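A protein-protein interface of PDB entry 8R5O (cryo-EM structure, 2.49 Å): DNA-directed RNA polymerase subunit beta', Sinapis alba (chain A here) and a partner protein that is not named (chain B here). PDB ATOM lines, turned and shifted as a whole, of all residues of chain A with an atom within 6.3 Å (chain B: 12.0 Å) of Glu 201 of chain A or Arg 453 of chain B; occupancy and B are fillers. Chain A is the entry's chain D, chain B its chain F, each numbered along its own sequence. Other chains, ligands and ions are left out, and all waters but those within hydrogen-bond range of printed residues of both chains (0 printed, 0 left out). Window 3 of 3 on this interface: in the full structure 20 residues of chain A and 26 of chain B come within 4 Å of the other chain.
Of the 17 printed residues of chain A, 4 touch a printed residue of chain B. Hydrophobic or aromatic side chains of chain A that line the printed part of chain B: Ala 204. Hydrophobic or aromatic side chains of chain B within 4 Å of the printed part of chain A: Pro 451. Among the printed residues, Asp or Glu carboxylates within 4 Å of a Lys or Arg side-chain nitrogen of the other chain: Glu 201 of chain A with Arg 453 of chain B (2.7 Å) and Asp 205 of chain A with Arg 453 of chain B (2.4 Å).
CB of Pro 451 of chain B touches NZ of Lys 153 of chain A, at 3.98 Å. Arg 452 of chain B touches Lys 153 of chain A (O to CE, 3.8 Å). Ala 204 of chain A touches Arg 453 of chain B (O to CG, 3.6 Å).
The guanidinium group (NH2) of Arg 453 of chain B lies within salt-bridge range of the side-chain carboxylate (OE1) of Glu 201 of chain A (2.7 Å). The side-chain carboxylate (OD1) of Asp 205 of chain A lies within salt-bridge range of the guanidinium group (NE) of Arg 453 of chain B (2.4 Å).
No residue of chain B comes within 4 Å of Pro 150 of chain A. Printed residues of chain B within 4 Å of Lys 153 of chain A: Pro 451 (3.98 Å) and Arg 452 (3.8 Å). No residue of chain B comes within 4 Å of Ala 198 of chain A. No residue of chain B comes within 4 Å of Arg 200 of chain A. Glu 201 of chain A touches just one residue of chain B: Arg 453. No residue of chain B comes within 4 Å of Gln 202 of chain A. No residue of chain B comes within 4 Å of Leu 203 of chain A. Of chain B, only Arg 453 comes within 4 Å of Ala 204 of chain A. Of the printed residues of chain B, Asp 205 of chain A touches Arg 453. No residue of chain B comes within 4 Å of Leu 206 of chain A. Printed residues of chain A within 4 Å of Arg 452 of chain B: Lys 153 (3.8 Å). Of chain A, only Glu 201, Ala 204 and Asp 205 come within 4 Å of Arg 453 of chain B. Thr 456 of chain B touches none of the printed residues of chain A. The nearest printed residue of chain A that does not touch Arg 453 of chain B is Lys 153 of chain A (4.1 Å). The nearest printed residue of chain A that does not touch Pro 451 of chain B is Asp 205 of chain A (7.4 Å).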
ATOM      1  N   PRO A 150      32.935   5.350   8.801  1.00  0.00           N
ATOM      2  CA  PRO A 150      31.980   4.263   8.537  1.00  0.00           C
ATOM      3  C   PRO A 150      31.158   3.875   9.752  1.00  0.00           C
ATOM      4  O   PRO A 150      30.040   3.371   9.594  1.00  0.00           O
ATOM      5  CB  PRO A 150      32.884   3.114   8.076  1.00  0.00           C
ATOM      6  CG  PRO A 150      34.169   3.368   8.769  1.00  0.00           C
ATOM      7  CD  PRO A 150      34.325   4.862   8.824  1.00  0.00           C
ATOM      8  N   ILE A 151      31.672   4.096  10.961  1.00  0.00           N
ATOM      9  CA  ILE A 151      31.021   3.646  12.182  1.00  0.00           C
ATOM     10  C   ILE A 151      30.680   4.856  13.041  1.00  0.00           C
ATOM     11  O   ILE A 151      31.227   5.949  12.870  1.00  0.00           O
ATOM     12  CB  ILE A 151      31.894   2.651  12.969  1.00  0.00           C
ATOM     13  CG1 ILE A 151      32.978   3.389  13.751  1.00  0.00           C
ATOM     14  CG2 ILE A 151      32.541   1.653  12.027  1.00  0.00           C
ATOM     15  CD1 ILE A 151      33.874   2.472  14.540  1.00  0.00           C
ATOM     16  N   LYS A 153      29.588   4.010  16.650  1.00  0.00           N
ATOM     17  CA  LYS A 153      29.498   3.489  18.006  1.00  0.00           C
ATOM     18  C   LYS A 153      30.847   3.430  18.712  1.00  0.00           C
ATOM     19  O   LYS A 153      30.942   2.837  19.790  1.00  0.00           O
ATOM     20  CB  LYS A 153      28.859   2.098  17.996  1.00  0.00           C
ATOM     21  CG  LYS A 153      27.432   2.076  17.479  1.00  0.00           C
ATOM     22  CD  LYS A 153      26.816   0.696  17.620  1.00  0.00           C
ATOM     23  CE  LYS A 153      25.452   0.635  16.956  1.00  0.00           C
ATOM     24  NZ  LYS A 153      24.536   1.691  17.468  1.00  0.00           N
ATOM     25  N   ASN A 189      40.681   1.545  10.572  1.00  0.00           N
ATOM     26  CA  ASN A 189      39.370   1.230  10.004  1.00  0.00           C
ATOM     27  C   ASN A 189      38.243   1.643  10.944  1.00  0.00           C
ATOM     28  O   ASN A 189      37.287   0.908  11.187  1.00  0.00           O
ATOM     29  CB  ASN A 189      39.292  -0.253   9.667  1.00  0.00           C
ATOM     30  CG  ASN A 189      40.318  -0.669   8.633  1.00  0.00           C
ATOM     31  OD1 ASN A 189      40.714   0.123   7.777  1.00  0.00           O
ATOM     32  ND2 ASN A 189      40.755  -1.921   8.706  1.00  0.00           N
ATOM     33  N   SER A 193      37.363   3.955   5.762  1.00  0.00           N
ATOM     34  CA  SER A 193      37.564   2.594   5.289  1.00  0.00           C
ATOM     35  C   SER A 193      37.255   2.520   3.800  1.00  0.00           C
ATOM     36  O   SER A 193      36.803   3.489   3.186  1.00  0.00           O
ATOM     37  CB  SER A 193      36.693   1.597   6.067  1.00  0.00           C
ATOM     38  OG  SER A 193      36.929   0.269   5.634  1.00  0.00           O
ATOM     39  N   ALA A 196      34.180  -3.420   0.147  1.00  0.00           N
ATOM     40  CA  ALA A 196      32.925  -3.957   0.662  1.00  0.00           C
ATOM     41  C   ALA A 196      32.946  -4.062   2.179  1.00  0.00           C
ATOM     42  O   ALA A 196      31.885  -4.060   2.815  1.00  0.00           O
ATOM     43  CB  ALA A 196      32.642  -5.323   0.038  1.00  0.00           C
ATOM     44  N   GLY A 197      34.136  -4.156   2.774  1.00  0.00           N
ATOM     45  CA  GLY A 197      34.232  -4.189   4.222  1.00  0.00           C
ATOM     46  C   GLY A 197      33.703  -2.933   4.883  1.00  0.00           C
ATOM     47  O   GLY A 197      33.117  -2.997   5.964  1.00  0.00           O
ATOM     48  N   ALA A 198      33.907  -1.777   4.249  1.00  0.00           N
ATOM     49  CA  ALA A 198      33.360  -0.533   4.783  1.00  0.00           C
ATOM     50  C   ALA A 198      31.838  -0.570   4.803  1.00  0.00           C
ATOM     51  O   ALA A 198      31.209  -0.064   5.739  1.00  0.00           O
ATOM     52  CB  ALA A 198      33.857   0.656   3.964  1.00  0.00           C
ATOM     53  N   ILE A 199      31.230  -1.162   3.774  1.00  0.00           N
ATOM     54  CA  ILE A 199      29.777  -1.283   3.730  1.00  0.00           C
ATOM     55  C   ILE A 199      29.275  -2.172   4.860  1.00  0.00           C
ATOM     56  O   ILE A 199      28.265  -1.868   5.504  1.00  0.00           O
ATOM     57  CB  ILE A 199      29.331  -1.807   2.353  1.00  0.00           C
ATOM     58  CG1 ILE A 199      29.616  -0.764   1.272  1.00  0.00           C
ATOM     59  CG2 ILE A 199      27.856  -2.179   2.367  1.00  0.00           C
ATOM     60  CD1 ILE A 199      29.152  -1.176  -0.097  1.00  0.00           C
ATOM     61  N   ARG A 200      29.972  -3.280   5.120  1.00  0.00           N
ATOM     62  CA  ARG A 200      29.539  -4.193   6.173  1.00  0.00           C
ATOM     63  C   ARG A 200      29.591  -3.526   7.541  1.00  0.00           C
ATOM     64  O   ARG A 200      28.735  -3.783   8.395  1.00  0.00           O
ATOM     65  CB  ARG A 200      30.395  -5.458   6.159  1.00  0.00           C
ATOM     66  CG  ARG A 200      29.763  -6.615   6.905  1.00  0.00           C
ATOM     67  CD  ARG A 200      30.568  -7.890   6.757  1.00  0.00           C
ATOM     68  NE  ARG A 200      29.791  -9.060   7.147  1.00  0.00           N
ATOM     69  CZ  ARG A 200      29.637  -9.475   8.397  1.00  0.00           C
ATOM     70  NH1 ARG A 200      30.200  -8.838   9.409  1.00  0.00           N
ATOM     71  NH2 ARG A 200      28.898 -10.554   8.635  1.00  0.00           N
ATOM     72  N   GLU A 201      30.590  -2.672   7.772  1.00  0.00           N
ATOM     73  CA  GLU A 201      30.646  -1.932   9.029  1.00  0.00           C
ATOM     74  C   GLU A 201      29.463  -0.983   9.162  1.00  0.00           C
ATOM     75  O   GLU A 201      28.904  -0.829  10.253  1.00  0.00           O
ATOM     76  CB  GLU A 201      31.964  -1.166   9.137  1.00  0.00           C
ATOM     77  CG  GLU A 201      33.200  -2.026   8.957  1.00  0.00           C
ATOM     78  CD  GLU A 201      33.240  -3.210   9.903  1.00  0.00           C
ATOM     79  OE1 GLU A 201      32.816  -3.060  11.068  1.00  0.00           O
ATOM     80  OE2 GLU A 201      33.696  -4.292   9.479  1.00  0.00           O
ATOM     81  N   GLN A 202      29.072  -0.331   8.065  1.00  0.00           N
ATOM     82  CA  GLN A 202      27.895   0.529   8.103  1.00  0.00           C
ATOM     83  C   GLN A 202      26.633  -0.276   8.384  1.00  0.00           C
ATOM     84  O   GLN A 202      25.788   0.142   9.184  1.00  0.00           O
ATOM     85  CB  GLN A 202      27.760   1.295   6.787  1.00  0.00           C
ATOM     86  CG  GLN A 202      28.973   2.133   6.429  1.00  0.00           C
ATOM     87  CD  GLN A 202      28.774   2.931   5.157  1.00  0.00           C
ATOM     88  OE1 GLN A 202      27.823   3.702   5.037  1.00  0.00           O
ATOM     89  NE2 GLN A 202      29.671   2.746   4.197  1.00  0.00           N
ATOM     90  N   LEU A 203      26.487  -1.435   7.737  1.00  0.00           N
ATOM     91  CA  LEU A 203      25.312  -2.270   7.970  1.00  0.00           C
ATOM     92  C   LEU A 203      25.276  -2.796   9.399  1.00  0.00           C
ATOM     93  O   LEU A 203      24.216  -2.807  10.035  1.00  0.00           O
ATOM     94  CB  LEU A 203      25.284  -3.431   6.975  1.00  0.00           C
ATOM     95  CG  LEU A 203      25.080  -3.070   5.504  1.00  0.00           C
ATOM     96  CD1 LEU A 203      25.298  -4.281   4.613  1.00  0.00           C
ATOM     97  CD2 LEU A 203      23.694  -2.489   5.292  1.00  0.00           C
ATOM     98  N   ALA A 204      26.422  -3.236   9.920  1.00  0.00           N
ATOM     99  CA  ALA A 204      26.458  -3.804  11.262  1.00  0.00           C
ATOM    100  C   ALA A 204      26.187  -2.754  12.332  1.00  0.00           C
ATOM    101  O   ALA A 204      25.651  -3.082  13.395  1.00  0.00           O
ATOM    102  CB  ALA A 204      27.805  -4.478  11.511  1.00  0.00           C
ATOM    103  N   ASP A 205      26.544  -1.498  12.074  1.00  0.00           N
ATOM    104  CA  ASP A 205      26.379  -0.422  13.042  1.00  0.00           C
ATOM    105  C   ASP A 205      25.076   0.343  12.870  1.00  0.00           C
ATOM    106  O   ASP A 205      24.861   1.335  13.573  1.00  0.00           O
ATOM    107  CB  ASP A 205      27.560   0.549  12.954  1.00  0.00           C
ATOM    108  CG  ASP A 205      28.851  -0.060  13.460  1.00  0.00           C
ATOM    109  OD1 ASP A 205      28.836  -0.675  14.545  1.00  0.00           O
ATOM    110  OD2 ASP A 205      29.880   0.068  12.767  1.00  0.00           O
ATOM    111  N   LEU A 206      24.207  -0.085  11.958  1.00  0.00           N
ATOM    112  CA  LEU A 206      22.936   0.597  11.759  1.00  0.00           C
ATOM    113  C   LEU A 206      22.038   0.440  12.979  1.00  0.00           C
ATOM    114  O   LEU A 206      21.950  -0.637  13.573  1.00  0.00           O
ATOM    115  CB  LEU A 206      22.223   0.051  10.524  1.00  0.00           C
ATOM    116  CG  LEU A 206      22.568   0.674   9.174  1.00  0.00           C
ATOM    117  CD1 LEU A 206      21.823  -0.043   8.068  1.00  0.00           C
ATOM    118  CD2 LEU A 206      22.234   2.156   9.173  1.00  0.00           C
ATOM    119  N   GLU A 262      23.823  -7.148   8.007  1.00  0.00           N
ATOM    120  CA  GLU A 262      25.224  -7.272   7.626  1.00  0.00           C
ATOM    121  C   GLU A 262      25.529  -8.580   6.910  1.00  0.00           C
ATOM    122  O   GLU A 262      26.612  -8.708   6.332  1.00  0.00           O
ATOM    123  CB  GLU A 262      26.133  -7.133   8.851  1.00  0.00           C
ATOM    124  CG  GLU A 262      25.780  -8.034  10.023  1.00  0.00           C
ATOM    125  CD  GLU A 262      24.780  -7.396  10.973  1.00  0.00           C
ATOM    126  OE1 GLU A 262      24.048  -6.480  10.545  1.00  0.00           O
ATOM    127  OE2 GLU A 262      24.730  -7.811  12.149  1.00  0.00           O
ATOM    128  N   LYS B 447      23.898  -0.071  34.941  1.00  0.00           N
ATOM    129  CA  LYS B 447      23.411  -0.025  33.567  1.00  0.00           C
ATOM    130  C   LYS B 447      24.300   0.919  32.765  1.00  0.00           C
ATOM    131  O   LYS B 447      24.303   2.132  32.998  1.00  0.00           O
ATOM    132  CB  LYS B 447      21.951   0.423  33.537  1.00  0.00           C
ATOM    133  CG  LYS B 447      21.464   0.947  32.194  1.00  0.00           C
ATOM    134  CD  LYS B 447      21.421  -0.140  31.138  1.00  0.00           C
ATOM    135  CE  LYS B 447      20.918   0.412  29.816  1.00  0.00           C
ATOM    136  NZ  LYS B 447      20.856  -0.636  28.764  1.00  0.00           N
ATOM    137  N   ARG B 448      25.060   0.362  31.825  1.00  0.00           N
ATOM    138  CA  ARG B 448      25.948   1.147  30.978  1.00  0.00           C
ATOM    139  C   ARG B 448      25.201   1.606  29.733  1.00  0.00           C
ATOM    140  O   ARG B 448      24.567   0.798  29.048  1.00  0.00           O
ATOM    141  CB  ARG B 448      27.178   0.332  30.578  1.00  0.00           C
ATOM    142  CG  ARG B 448      28.373   0.482  31.504  1.00  0.00           C
ATOM    143  CD  ARG B 448      28.119  -0.125  32.869  1.00  0.00           C
ATOM    144  NE  ARG B 448      29.336  -0.166  33.668  1.00  0.00           N
ATOM    145  CZ  ARG B 448      30.183  -1.186  33.688  1.00  0.00           C
ATOM    146  NH1 ARG B 448      29.965  -2.279  32.977  1.00  0.00           N
ATOM    147  NH2 ARG B 448      31.276  -1.107  34.442  1.00  0.00           N
ATOM    148  N   TRP B 449      25.280   2.899  29.443  1.00  0.00           N
ATOM    149  CA  TRP B 449      24.644   3.471  28.258  1.00  0.00           C
ATOM    150  C   TRP B 449      25.643   3.566  27.106  1.00  0.00           C
ATOM    151  O   TRP B 449      25.911   4.632  26.557  1.00  0.00           O
ATOM    152  CB  TRP B 449      24.041   4.831  28.591  1.00  0.00           C
ATOM    153  CG  TRP B 449      22.912   4.741  29.566  1.00  0.00           C
ATOM    154  CD1 TRP B 449      23.007   4.588  30.916  1.00  0.00           C
ATOM    155  CD2 TRP B 449      21.514   4.788  29.264  1.00  0.00           C
ATOM    156  NE1 TRP B 449      21.756   4.540  31.476  1.00  0.00           N
ATOM    157  CE2 TRP B 449      20.820   4.661  30.482  1.00  0.00           C
ATOM    158  CE3 TRP B 449      20.782   4.928  28.082  1.00  0.00           C
ATOM    159  CZ2 TRP B 449      19.429   4.669  30.553  1.00  0.00           C
ATOM    160  CZ3 TRP B 449      19.400   4.937  28.154  1.00  0.00           C
ATOM    161  CH2 TRP B 449      18.739   4.808  29.381  1.00  0.00           C
ATOM    162  N   VAL B 450      26.191   2.415  26.746  1.00  0.00           N
ATOM    163  CA  VAL B 450      27.167   2.280  25.670  1.00  0.00           C
ATOM    164  C   VAL B 450      26.476   1.612  24.486  1.00  0.00           C
ATOM    165  O   VAL B 450      26.030   0.465  24.610  1.00  0.00           O
ATOM    166  CB  VAL B 450      28.395   1.472  26.116  1.00  0.00           C
ATOM    167  CG1 VAL B 450      29.357   1.288  24.957  1.00  0.00           C
ATOM    168  CG2 VAL B 450      29.081   2.156  27.284  1.00  0.00           C
ATOM    169  N   PRO B 451      26.345   2.285  23.345  1.00  0.00           N
ATOM    170  CA  PRO B 451      25.739   1.639  22.174  1.00  0.00           C
ATOM    171  C   PRO B 451      26.545   0.427  21.732  1.00  0.00           C
ATOM    172  O   PRO B 451      27.777   0.434  21.752  1.00  0.00           O
ATOM    173  CB  PRO B 451      25.757   2.744  21.111  1.00  0.00           C
ATOM    174  CG  PRO B 451      25.865   4.019  21.884  1.00  0.00           C
ATOM    175  CD  PRO B 451      26.693   3.690  23.083  1.00  0.00           C
ATOM    176  N   ARG B 452      25.834  -0.624  21.330  1.00  0.00           N
ATOM    177  CA  ARG B 452      26.465  -1.860  20.898  1.00  0.00           C
ATOM    178  C   ARG B 452      25.749  -2.394  19.668  1.00  0.00           C
ATOM    179  O   ARG B 452      24.585  -2.078  19.412  1.00  0.00           O
ATOM    180  CB  ARG B 452      26.467  -2.917  22.012  1.00  0.00           C
ATOM    181  CG  ARG B 452      27.265  -2.517  23.240  1.00  0.00           C
ATOM    182  CD  ARG B 452      27.853  -3.727  23.941  1.00  0.00           C
ATOM    183  NE  ARG B 452      28.727  -3.340  25.041  1.00  0.00           N
ATOM    184  CZ  ARG B 452      29.989  -2.959  24.896  1.00  0.00           C
ATOM    185  NH1 ARG B 452      30.560  -2.897  23.704  1.00  0.00           N
ATOM    186  NH2 ARG B 452      30.696  -2.630  25.973  1.00  0.00           N
ATOM    187  N   ARG B 453      26.467  -3.211  18.903  1.00  0.00           N
ATOM    188  CA  ARG B 453      25.906  -3.801  17.696  1.00  0.00           C
ATOM    189  C   ARG B 453      24.907  -4.894  18.052  1.00  0.00           C
ATOM    190  O   ARG B 453      25.175  -5.741  18.911  1.00  0.00           O
ATOM    191  CB  ARG B 453      27.019  -4.364  16.815  1.00  0.00           C
ATOM    192  CG  ARG B 453      27.908  -3.302  16.196  1.00  0.00           C
ATOM    193  CD  ARG B 453      28.984  -3.920  15.323  1.00  0.00           C
ATOM    194  NE  ARG B 453      29.740  -2.906  14.600  1.00  0.00           N
ATOM    195  CZ  ARG B 453      30.765  -3.164  13.799  1.00  0.00           C
ATOM    196  NH1 ARG B 453      31.189  -4.400  13.598  1.00  0.00           N
ATOM    197  NH2 ARG B 453      31.378  -2.156  13.187  1.00  0.00           N
ATOM    198  N   GLY B 454      23.763  -4.874  17.394  1.00  0.00           N
ATOM    199  CA  GLY B 454      22.701  -5.834  17.632  1.00  0.00           C
ATOM    200  C   GLY B 454      21.349  -5.149  17.620  1.00  0.00           C
ATOM    201  O   GLY B 454      21.225  -3.939  17.809  1.00  0.00           O
ATOM    202  N   LYS B 455      20.309  -5.945  17.386  1.00  0.00           N
ATOM    203  CA  LYS B 455      18.939  -5.436  17.335  1.00  0.00           C
ATOM    204  C   LYS B 455      18.255  -5.530  18.697  1.00  0.00           C
ATOM    205  O   LYS B 455      17.141  -6.033  18.833  1.00  0.00           O
ATOM    206  CB  LYS B 455      18.150  -6.185  16.268  1.00  0.00           C
ATOM    207  CG  LYS B 455      18.246  -7.699  16.375  1.00  0.00           C
ATOM    208  CD  LYS B 455      17.509  -8.385  15.238  1.00  0.00           C
ATOM    209  CE  LYS B 455      18.140  -8.068  13.894  1.00  0.00           C
ATOM    210  NZ  LYS B 455      17.456  -8.782  12.783  1.00  0.00           N
ATOM    211  N   THR B 456      18.935  -5.026  19.724  1.00  0.00           N
ATOM    212  CA  THR B 456      18.404  -4.991  21.082  1.00  0.00           C
ATOM    213  C   THR B 456      18.486  -3.549  21.561  1.00  0.00           C
ATOM    214  O   THR B 456      19.601  -2.995  21.657  1.00  0.00           O
ATOM    215  CB  THR B 456      19.177  -5.924  22.015  1.00  0.00           C
ATOM    216  OG1 THR B 456      19.127  -7.261  21.504  1.00  0.00           O
ATOM    217  CG2 THR B 456      18.571  -5.900  23.408  1.00  0.00           C
ATOM    218  N   PRO B 457      17.363  -2.901  21.856  1.00  0.00           N
ATOM    219  CA  PRO B 457      17.404  -1.479  22.209  1.00  0.00           C
ATOM    220  C   PRO B 457      18.158  -1.229  23.506  1.00  0.00           C
ATOM    221  O   PRO B 457      18.113  -2.025  24.447  1.00  0.00           O
ATOM    222  CB  PRO B 457      15.924  -1.105  22.345  1.00  0.00           C
ATOM    223  CG  PRO B 457      15.243  -2.390  22.663  1.00  0.00           C
ATOM    224  CD  PRO B 457      15.999  -3.451  21.925  1.00  0.00           C
ATOM    225  N   LEU B 458      18.864  -0.098  23.538  1.00  0.00           N
ATOM    226  CA  LEU B 458      19.582   0.311  24.739  1.00  0.00           C
ATOM    227  C   LEU B 458      18.645   0.886  25.794  1.00  0.00           C
ATOM    228  O   LEU B 458      18.888   0.714  26.993  1.00  0.00           O
ATOM    229  CB  LEU B 458      20.662   1.332  24.377  1.00  0.00           C
ATOM    230  CG  LEU B 458      21.613   1.794  25.483  1.00  0.00           C
ATOM    231  CD1 LEU B 458      22.461   0.638  25.983  1.00  0.00           C
ATOM    232  CD2 LEU B 458      22.488   2.933  24.989  1.00  0.00           C
ATOM    233  N   ASP B 459      17.583   1.558  25.372  1.00  0.00           N
ATOM    234  CA  ASP B 459      16.650   2.163  26.313  1.00  0.00           C
ATOM    235  C   ASP B 459      15.806   1.081  26.978  1.00  0.00           C
ATOM    236  O   ASP B 459      15.145   0.303  26.280  1.00  0.00           O
ATOM    237  CB  ASP B 459      15.758   3.166  25.582  1.00  0.00           C
ATOM    238  CG  ASP B 459      14.901   3.991  26.523  1.00  0.00           C
ATOM    239  OD1 ASP B 459      15.121   3.932  27.749  1.00  0.00           O
ATOM    240  OD2 ASP B 459      14.003   4.704  26.030  1.00  0.00           O
